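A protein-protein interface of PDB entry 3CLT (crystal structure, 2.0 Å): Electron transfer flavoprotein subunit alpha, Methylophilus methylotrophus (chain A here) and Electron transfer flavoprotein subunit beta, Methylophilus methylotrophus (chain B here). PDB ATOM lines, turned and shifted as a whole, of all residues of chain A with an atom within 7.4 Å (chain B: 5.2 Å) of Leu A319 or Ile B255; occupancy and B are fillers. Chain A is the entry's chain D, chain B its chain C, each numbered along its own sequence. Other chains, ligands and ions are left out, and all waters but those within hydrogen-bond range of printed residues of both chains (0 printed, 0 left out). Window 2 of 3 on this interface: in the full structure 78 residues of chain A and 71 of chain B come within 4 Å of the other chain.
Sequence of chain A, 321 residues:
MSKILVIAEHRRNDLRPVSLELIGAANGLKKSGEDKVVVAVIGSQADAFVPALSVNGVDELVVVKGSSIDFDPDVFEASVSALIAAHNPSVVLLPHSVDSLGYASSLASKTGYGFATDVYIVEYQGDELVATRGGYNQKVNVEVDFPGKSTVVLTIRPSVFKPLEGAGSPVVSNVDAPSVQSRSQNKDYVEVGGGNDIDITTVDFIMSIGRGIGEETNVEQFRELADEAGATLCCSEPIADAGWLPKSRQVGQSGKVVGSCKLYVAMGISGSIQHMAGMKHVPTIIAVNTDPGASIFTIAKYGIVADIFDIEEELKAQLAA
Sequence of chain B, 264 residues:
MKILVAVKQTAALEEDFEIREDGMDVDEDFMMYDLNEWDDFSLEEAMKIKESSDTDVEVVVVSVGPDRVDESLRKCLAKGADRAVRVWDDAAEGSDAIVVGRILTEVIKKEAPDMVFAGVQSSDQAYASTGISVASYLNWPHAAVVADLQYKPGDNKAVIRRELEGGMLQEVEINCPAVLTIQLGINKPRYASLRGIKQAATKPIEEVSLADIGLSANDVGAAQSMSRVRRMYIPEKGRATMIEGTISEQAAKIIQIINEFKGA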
ATOM      1  N   PHE A 205     -29.821  40.388 -19.822  1.00  0.00           N
ATOM      2  CA  PHE A 205     -29.221  39.055 -19.921  1.00  0.00           C
ATOM      3  C   PHE A 205     -29.141  38.674 -21.393  1.00  0.00           C
ATOM      4  O   PHE A 205     -30.158  38.426 -22.042  1.00  0.00           O
ATOM      5  CB  PHE A 205     -30.037  38.041 -19.089  1.00  0.00           C
ATOM      6  CG  PHE A 205     -29.519  36.602 -19.121  1.00  0.00           C
ATOM      7  CD1 PHE A 205     -30.362  35.563 -18.753  1.00  0.00           C
ATOM      8  CD2 PHE A 205     -28.216  36.281 -19.495  1.00  0.00           C
ATOM      9  CE1 PHE A 205     -29.924  34.242 -18.766  1.00  0.00           C
ATOM     10  CE2 PHE A 205     -27.778  34.952 -19.515  1.00  0.00           C
ATOM     11  CZ  PHE A 205     -28.637  33.939 -19.149  1.00  0.00           C
ATOM     12  N   MET A 207     -27.209  36.294 -24.499  1.00  0.00           N
ATOM     13  CA  MET A 207     -26.362  35.260 -25.080  1.00  0.00           C
ATOM     14  C   MET A 207     -26.073  35.707 -26.511  1.00  0.00           C
ATOM     15  O   MET A 207     -26.993  35.991 -27.275  1.00  0.00           O
ATOM     16  CB  MET A 207     -27.072  33.915 -25.048  1.00  0.00           C
ATOM     17  CG  MET A 207     -27.070  33.262 -23.668  1.00  0.00           C
ATOM     18  SD  MET A 207     -28.021  31.753 -23.602  1.00  0.00           S
ATOM     19  CE  MET A 207     -27.539  31.124 -22.004  1.00  0.00           C
ATOM     20  N   GLU A 224     -32.827  28.576 -29.218  1.00  0.00           N
ATOM     21  CA  GLU A 224     -33.521  27.699 -28.284  1.00  0.00           C
ATOM     22  C   GLU A 224     -32.899  27.803 -26.892  1.00  0.00           C
ATOM     23  O   GLU A 224     -33.616  27.872 -25.893  1.00  0.00           O
ATOM     24  CB  GLU A 224     -33.493  26.245 -28.785  1.00  0.00           C
ATOM     25  CG  GLU A 224     -34.309  26.023 -30.078  1.00  0.00           C
ATOM     26  CD  GLU A 224     -34.188  24.609 -30.664  1.00  0.00           C
ATOM     27  OE1 GLU A 224     -33.381  23.805 -30.156  1.00  0.00           O
ATOM     28  OE2 GLU A 224     -34.901  24.304 -31.650  1.00  0.00           O
ATOM     29  N   LEU A 225     -31.570  27.809 -26.837  1.00  0.00           N
ATOM     30  CA  LEU A 225     -30.848  27.960 -25.572  1.00  0.00           C
ATOM     31  C   LEU A 225     -31.190  29.285 -24.893  1.00  0.00           C
ATOM     32  O   LEU A 225     -31.472  29.311 -23.690  1.00  0.00           O
ATOM     33  CB  LEU A 225     -29.332  27.862 -25.788  1.00  0.00           C
ATOM     34  CG  LEU A 225     -28.459  28.131 -24.546  1.00  0.00           C
ATOM     35  CD1 LEU A 225     -28.651  27.066 -23.497  1.00  0.00           C
ATOM     36  CD2 LEU A 225     -26.988  28.253 -24.907  1.00  0.00           C
ATOM     37  N   ALA A 226     -31.148  30.370 -25.670  1.00  0.00           N
ATOM     38  CA  ALA A 226     -31.484  31.715 -25.187  1.00  0.00           C
ATOM     39  C   ALA A 226     -32.892  31.764 -24.602  1.00  0.00           C
ATOM     40  O   ALA A 226     -33.104  32.286 -23.498  1.00  0.00           O
ATOM     41  CB  ALA A 226     -31.345  32.724 -26.310  1.00  0.00           C
ATOM     42  N   ASP A 227     -33.847  31.199 -25.339  1.00  0.00           N
ATOM     43  CA  ASP A 227     -35.228  31.111 -24.883  1.00  0.00           C
ATOM     44  C   ASP A 227     -35.377  30.296 -23.590  1.00  0.00           C
ATOM     45  O   ASP A 227     -36.082  30.716 -22.674  1.00  0.00           O
ATOM     46  CB  ASP A 227     -36.112  30.503 -25.977  1.00  0.00           C
ATOM     47  CG  ASP A 227     -36.319  31.439 -27.154  1.00  0.00           C
ATOM     48  OD1 ASP A 227     -35.783  32.571 -27.126  1.00  0.00           O
ATOM     49  OD2 ASP A 227     -37.026  31.041 -28.113  1.00  0.00           O
ATOM     50  N   GLU A 228     -34.719  29.142 -23.518  1.00  0.00           N
ATOM     51  CA  GLU A 228     -34.785  28.297 -22.323  1.00  0.00           C
ATOM     52  C   GLU A 228     -34.155  28.989 -21.101  1.00  0.00           C
ATOM     53  O   GLU A 228     -34.601  28.788 -19.973  1.00  0.00           O
ATOM     54  CB  GLU A 228     -34.116  26.939 -22.575  1.00  0.00           C
ATOM     55  N   ALA A 229     -33.140  29.813 -21.344  1.00  0.00           N
ATOM     56  CA  ALA A 229     -32.405  30.514 -20.286  1.00  0.00           C
ATOM     57  C   ALA A 229     -33.044  31.830 -19.869  1.00  0.00           C
ATOM     58  O   ALA A 229     -32.731  32.340 -18.793  1.00  0.00           O
ATOM     59  CB  ALA A 229     -30.966  30.778 -20.733  1.00  0.00           C
ATOM     60  N   GLY A 230     -33.916  32.382 -20.718  1.00  0.00           N
ATOM     61  CA  GLY A 230     -34.494  33.710 -20.498  1.00  0.00           C
ATOM     62  C   GLY A 230     -33.517  34.821 -20.854  1.00  0.00           C
ATOM     63  O   GLY A 230     -33.529  35.888 -20.234  1.00  0.00           O
ATOM     64  N   ILE A 286     -19.151  36.001 -19.616  1.00  0.00           N
ATOM     65  CA  ILE A 286     -18.687  34.625 -19.808  1.00  0.00           C
ATOM     66  C   ILE A 286     -18.311  34.459 -21.274  1.00  0.00           C
ATOM     67  O   ILE A 286     -19.086  34.809 -22.157  1.00  0.00           O
ATOM     68  CB  ILE A 286     -19.791  33.588 -19.453  1.00  0.00           C
ATOM     69  CG1 ILE A 286     -20.306  33.812 -18.033  1.00  0.00           C
ATOM     70  CG2 ILE A 286     -19.268  32.151 -19.622  1.00  0.00           C
ATOM     71  CD1 ILE A 286     -21.531  32.991 -17.685  1.00  0.00           C
ATOM     72  N   GLU A 312     -23.477  24.321 -25.561  1.00  0.00           N
ATOM     73  CA  GLU A 312     -24.894  24.657 -25.760  1.00  0.00           C
ATOM     74  C   GLU A 312     -25.835  23.473 -25.474  1.00  0.00           C
ATOM     75  O   GLU A 312     -26.847  23.616 -24.779  1.00  0.00           O
ATOM     76  CB  GLU A 312     -25.103  25.203 -27.178  1.00  0.00           C
ATOM     77  CG  GLU A 312     -26.550  25.483 -27.556  1.00  0.00           C
ATOM     78  CD  GLU A 312     -27.299  24.252 -28.004  1.00  0.00           C
ATOM     79  OE1 GLU A 312     -26.749  23.460 -28.800  1.00  0.00           O
ATOM     80  OE2 GLU A 312     -28.448  24.069 -27.556  1.00  0.00           O
ATOM     81  N   GLU A 313     -25.518  22.301 -26.010  1.00  0.00           N
ATOM     82  CA  GLU A 313     -26.403  21.153 -25.821  1.00  0.00           C
ATOM     83  C   GLU A 313     -26.460  20.719 -24.340  1.00  0.00           C
ATOM     84  O   GLU A 313     -27.541  20.436 -23.815  1.00  0.00           O
ATOM     85  CB  GLU A 313     -26.071  20.005 -26.794  1.00  0.00           C
ATOM     86  CG  GLU A 313     -24.862  19.142 -26.451  1.00  0.00           C
ATOM     87  CD  GLU A 313     -24.768  17.859 -27.304  1.00  0.00           C
ATOM     88  OE1 GLU A 313     -25.820  17.244 -27.634  1.00  0.00           O
ATOM     89  OE2 GLU A 313     -23.621  17.460 -27.634  1.00  0.00           O
ATOM     90  N   GLU A 314     -25.315  20.720 -23.659  1.00  0.00           N
ATOM     91  CA  GLU A 314     -25.271  20.345 -22.233  1.00  0.00           C
ATOM     92  C   GLU A 314     -25.996  21.369 -21.363  1.00  0.00           C
ATOM     93  O   GLU A 314     -26.689  21.015 -20.411  1.00  0.00           O
ATOM     94  CB  GLU A 314     -23.826  20.188 -21.764  1.00  0.00           C
ATOM     95  CG  GLU A 314     -23.653  19.726 -20.323  1.00  0.00           C
ATOM     96  CD  GLU A 314     -24.225  18.338 -20.050  1.00  0.00           C
ATOM     97  OE1 GLU A 314     -24.282  17.503 -20.980  1.00  0.00           O
ATOM     98  OE2 GLU A 314     -24.608  18.073 -18.895  1.00  0.00           O
ATOM     99  N   LEU A 315     -25.827  22.641 -21.704  1.00  0.00           N
ATOM    100  CA  LEU A 315     -26.503  23.731 -21.011  1.00  0.00           C
ATOM    101  C   LEU A 315     -28.018  23.553 -21.126  1.00  0.00           C
ATOM    102  O   LEU A 315     -28.735  23.567 -20.110  1.00  0.00           O
ATOM    103  CB  LEU A 315     -26.063  25.068 -21.624  1.00  0.00           C
ATOM    104  CG  LEU A 315     -25.779  26.311 -20.798  1.00  0.00           C
ATOM    105  CD1 LEU A 315     -25.277  26.034 -19.376  1.00  0.00           C
ATOM    106  CD2 LEU A 315     -24.788  27.163 -21.586  1.00  0.00           C
ATOM    107  N   LYS A 316     -28.496  23.355 -22.357  1.00  0.00           N
ATOM    108  CA  LYS A 316     -29.927  23.144 -22.610  1.00  0.00           C
ATOM    109  C   LYS A 316     -30.485  21.996 -21.793  1.00  0.00           C
ATOM    110  O   LYS A 316     -31.542  22.133 -21.173  1.00  0.00           O
ATOM    111  CB  LYS A 316     -30.211  22.905 -24.100  1.00  0.00           C
ATOM    112  N   ALA A 317     -29.773  20.869 -21.788  1.00  0.00           N
ATOM    113  CA  ALA A 317     -30.209  19.686 -21.064  1.00  0.00           C
ATOM    114  C   ALA A 317     -30.274  19.932 -19.551  1.00  0.00           C
ATOM    115  O   ALA A 317     -31.230  19.531 -18.888  1.00  0.00           O
ATOM    116  CB  ALA A 317     -29.287  18.518 -21.374  1.00  0.00           C
ATOM    117  N   GLN A 318     -29.257  20.592 -19.009  1.00  0.00           N
ATOM    118  CA  GLN A 318     -29.235  20.915 -17.583  1.00  0.00           C
ATOM    119  C   GLN A 318     -30.321  21.924 -17.196  1.00  0.00           C
ATOM    120  O   GLN A 318     -30.906  21.819 -16.117  1.00  0.00           O
ATOM    121  CB  GLN A 318     -27.849  21.411 -17.162  1.00  0.00           C
ATOM    122  CG  GLN A 318     -26.819  20.286 -17.094  1.00  0.00           C
ATOM    123  CD  GLN A 318     -25.470  20.724 -16.557  1.00  0.00           C
ATOM    124  OE1 GLN A 318     -25.371  21.686 -15.808  1.00  0.00           O
ATOM    125  NE2 GLN A 318     -24.426  19.998 -16.925  1.00  0.00           N
ATOM    126  N   LEU A 319     -30.606  22.883 -18.077  1.00  0.00           N
ATOM    127  CA  LEU A 319     -31.660  23.870 -17.817  1.00  0.00           C
ATOM    128  C   LEU A 319     -33.065  23.251 -17.763  1.00  0.00           C
ATOM    129  O   LEU A 319     -33.946  23.799 -17.113  1.00  0.00           O
ATOM    130  CB  LEU A 319     -31.634  24.996 -18.860  1.00  0.00           C
ATOM    131  CG  LEU A 319     -30.548  26.060 -18.719  1.00  0.00           C
ATOM    132  CD1 LEU A 319     -30.437  26.865 -20.000  1.00  0.00           C
ATOM    133  CD2 LEU A 319     -30.817  26.991 -17.543  1.00  0.00           C
ATOM    134  N   ALA A 320     -33.262  22.118 -18.436  1.00  0.00           N
ATOM    135  CA  ALA A 320     -34.574  21.459 -18.523  1.00  0.00           C
ATOM    136  C   ALA A 320     -34.837  20.510 -17.350  1.00  0.00           C
ATOM    137  O   ALA A 320     -33.984  19.694 -16.976  1.00  0.00           O
ATOM    138  CB  ALA A 320     -34.689  20.701 -19.849  1.00  0.00           C
ATOM    139  N   ALA B 251     -20.714  23.505 -18.087  1.00  0.00           N
ATOM    140  CA  ALA B 251     -22.119  23.894 -18.163  1.00  0.00           C
ATOM    141  C   ALA B 251     -22.736  24.115 -16.777  1.00  0.00           C
ATOM    142  O   ALA B 251     -23.518  25.039 -16.592  1.00  0.00           O
ATOM    143  CB  ALA B 251     -22.919  22.854 -18.940  1.00  0.00           C
ATOM    144  N   ALA B 252     -22.385  23.269 -15.810  1.00  0.00           N
ATOM    145  CA  ALA B 252     -22.898  23.415 -14.448  1.00  0.00           C
ATOM    146  C   ALA B 252     -22.460  24.745 -13.803  1.00  0.00           C
ATOM    147  O   ALA B 252     -23.240  25.386 -13.089  1.00  0.00           O
ATOM    148  CB  ALA B 252     -22.473  22.218 -13.582  1.00  0.00           C
ATOM    149  N   LYS B 253     -21.224  25.160 -14.061  1.00  0.00           N
ATOM    150  CA  LYS B 253     -20.723  26.421 -13.530  1.00  0.00           C
ATOM    151  C   LYS B 253     -21.433  27.611 -14.164  1.00  0.00           C
ATOM    152  O   LYS B 253     -21.769  28.571 -13.476  1.00  0.00           O
ATOM    153  CB  LYS B 253     -19.208  26.526 -13.726  1.00  0.00           C
ATOM    154  CG  LYS B 253     -18.578  27.812 -13.205  1.00  0.00           C
ATOM    155  CD  LYS B 253     -18.755  28.001 -11.722  1.00  0.00           C
ATOM    156  CE  LYS B 253     -18.138  29.319 -11.291  1.00  0.00           C
ATOM    157  NZ  LYS B 253     -18.290  29.533  -9.835  1.00  0.00           N
ATOM    158  N   ILE B 254     -21.668  27.544 -15.473  1.00  0.00           N
ATOM    159  CA  ILE B 254     -22.386  28.604 -16.175  1.00  0.00           C
ATOM    160  C   ILE B 254     -23.776  28.781 -15.576  1.00  0.00           C
ATOM    161  O   ILE B 254     -24.205  29.901 -15.326  1.00  0.00           O
ATOM    162  CB  ILE B 254     -22.496  28.334 -17.700  1.00  0.00           C
ATOM    163  CG1 ILE B 254     -21.115  28.447 -18.362  1.00  0.00           C
ATOM    164  CG2 ILE B 254     -23.460  29.325 -18.358  1.00  0.00           C
ATOM    165  CD1 ILE B 254     -21.058  27.917 -19.790  1.00  0.00           C
ATOM    166  N   ILE B 255     -24.467  27.675 -15.327  1.00  0.00           N
ATOM    167  CA  ILE B 255     -25.803  27.735 -14.745  1.00  0.00           C
ATOM    168  C   ILE B 255     -25.791  28.354 -13.345  1.00  0.00           C
ATOM    169  O   ILE B 255     -26.696  29.107 -12.990  1.00  0.00           O
ATOM    170  CB  ILE B 255     -26.476  26.346 -14.745  1.00  0.00           C
ATOM    171  CG1 ILE B 255     -26.879  26.005 -16.184  1.00  0.00           C
ATOM    172  CG2 ILE B 255     -27.693  26.320 -13.803  1.00  0.00           C
ATOM    173  CD1 ILE B 255     -27.518  24.654 -16.369  1.00  0.00           C
ATOM    174  N   GLN B 256     -24.772  28.041 -12.558  1.00  0.00           N
ATOM    175  CA  GLN B 256     -24.639  28.642 -11.234  1.00  0.00           C
ATOM    176  C   GLN B 256     -24.431  30.142 -11.329  1.00  0.00           C
ATOM    177  O   GLN B 256     -25.008  30.894 -10.559  1.00  0.00           O
ATOM    178  CB  GLN B 256     -23.501  27.996 -10.469  1.00  0.00           C
ATOM    179  CG  GLN B 256     -23.834  26.580 -10.079  1.00  0.00           C
ATOM    180  CD  GLN B 256     -22.869  26.000  -9.084  1.00  0.00           C
ATOM    181  OE1 GLN B 256     -23.085  24.901  -8.575  1.00  0.00           O
ATOM    182  NE2 GLN B 256     -21.801  26.737  -8.792  1.00  0.00           N
ATOM    183  N   ILE B 257     -23.619  30.565 -12.295  1.00  0.00           N
ATOM    184  CA  ILE B 257     -23.437  31.985 -12.588  1.00  0.00           C
ATOM    185  C   ILE B 257     -24.748  32.629 -13.046  1.00  0.00           C
ATOM    186  O   ILE B 257     -25.094  33.717 -12.590  1.00  0.00           O
ATOM    187  CB  ILE B 257     -22.340  32.218 -13.655  1.00  0.00           C
ATOM    188  CG1 ILE B 257     -20.985  31.717 -13.147  1.00  0.00           C
ATOM    189  CG2 ILE B 257     -22.253  33.698 -14.012  1.00  0.00           C
ATOM    190  CD1 ILE B 257     -19.989  31.388 -14.277  1.00  0.00           C
ATOM    191  N   ILE B 258     -25.482  31.958 -13.932  1.00  0.00           N
ATOM    192  CA  ILE B 258     -26.806  32.442 -14.348  1.00  0.00           C
ATOM    193  C   ILE B 258     -27.739  32.609 -13.152  1.00  0.00           C
ATOM    194  O   ILE B 258     -28.399  33.637 -13.015  1.00  0.00           O
ATOM    195  CB  ILE B 258     -27.463  31.501 -15.389  1.00  0.00           C
ATOM    196  CG1 ILE B 258     -26.715  31.587 -16.721  1.00  0.00           C
ATOM    197  CG2 ILE B 258     -28.941  31.851 -15.600  1.00  0.00           C
ATOM    198  CD1 ILE B 258     -27.070  30.474 -17.693  1.00  0.00           C
ATOM    199  N   ASN B 259     -27.799  31.592 -12.297  1.00  0.00           N
ATOM    200  CA  ASN B 259     -28.647  31.642 -11.109  1.00  0.00           C
ATOM    201  C   ASN B 259     -28.226  32.732 -10.129  1.00  0.00           C
ATOM    202  O   ASN B 259     -29.080  33.374  -9.522  1.00  0.00           O
ATOM    203  CB  ASN B 259     -28.670  30.282 -10.397  1.00  0.00           C
ATOM    204  CG  ASN B 259     -29.382  29.203 -11.209  1.00  0.00           C
ATOM    205  OD1 ASN B 259     -30.190  29.495 -12.095  1.00  0.00           O
ATOM    206  ND2 ASN B 259     -29.074  27.947 -10.906  1.00  0.00           N
ATOM    207  N   GLU B 260     -26.921  32.952  -9.977  1.00  0.00           N
ATOM    208  CA  GLU B 260     -26.446  34.024  -9.102  1.00  0.00           C
ATOM    209  C   GLU B 260     -26.978  35.355  -9.636  1.00  0.00           C
ATOM    210  O   GLU B 260     -27.534  36.158  -8.880  1.00  0.00           O
ATOM    211  CB  GLU B 260     -24.918  34.038  -8.990  1.00  0.00           C
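N of Ala B252 sits close to OE1 of Gln A318, 3.4 Å away.
The side-chain carboxylate (OE2) of Glu A314 lies within hydrogen-bond range of the side-chain amide nitrogen (NE2) of Gln A318 (2.8 Å). The backbone carbonyl oxygen of Ile B255 sits close to the side-chain amide nitrogen of Asn B259, 3.4 Å away.
Among the printed residues, merely in contact across the chains: Phe A205 with Ile B258 (3.9 Å), Ile A286 with Ile B257 (3.8 Å), Glu A314 with Ala B251 (3.5 Å), Leu A315 with Ala B251 (3.4 Å), Leu A315 with Ile B254 (3.9 Å), Leu A315 with Ile B255 (3.6 Å), Gln A318 with Ala B251 (3.7 Å), Gln A318 with Ile B255 (3.4 Å) and Leu A319 with Ile B255 (3.9 Å).
Leu A319 touches just one residue of chain B: Ile B255 (3.9 Å). Printed residues of chain A within 4 Å of Ile B258: Phe A205. Printed residues of chain A within 4 Å of Ile B254: Leu A315. Printed residues of chain B within 4 Å of Ile A286: Ile B257 (3.8 Å). Of the printed residues of chain B, Leu A315 touches Ala B251, Ile B254 and Ile B255. Printed residues of chain B within 4 Å of Glu A314: Ala B251 (3.5 Å). Gly A230 touches none of the printed residues of chain B. Ala A320 touches none of the printed residues of chain B. The nearest residue of chain A that does not touch Ile B255 is Glu A314 (5.5 Å). The nearest printed residue of chain A that does not touch Ile B254 is Ile A286 (4.2 Å).
Of the 19 printed residues of chain A, 6 touch a printed residue of chain B. Printed residues of chain A that touch a printed residue of chain B: Phe A205, Ile A286, Glu A314, Leu A315, Gln A318 and Leu A319. Hydrophobic or aromatic side chains of chain A within 4 Å of the printed part of chain B: Phe A205, Ile A286 and Leu A315. Hydrophobic or aromatic side chains of chain B within 4 Å of the printed part of chain A: Ala B251, Ala B252, Ile B254, Ile B255, Ile B257 and Ile B258.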
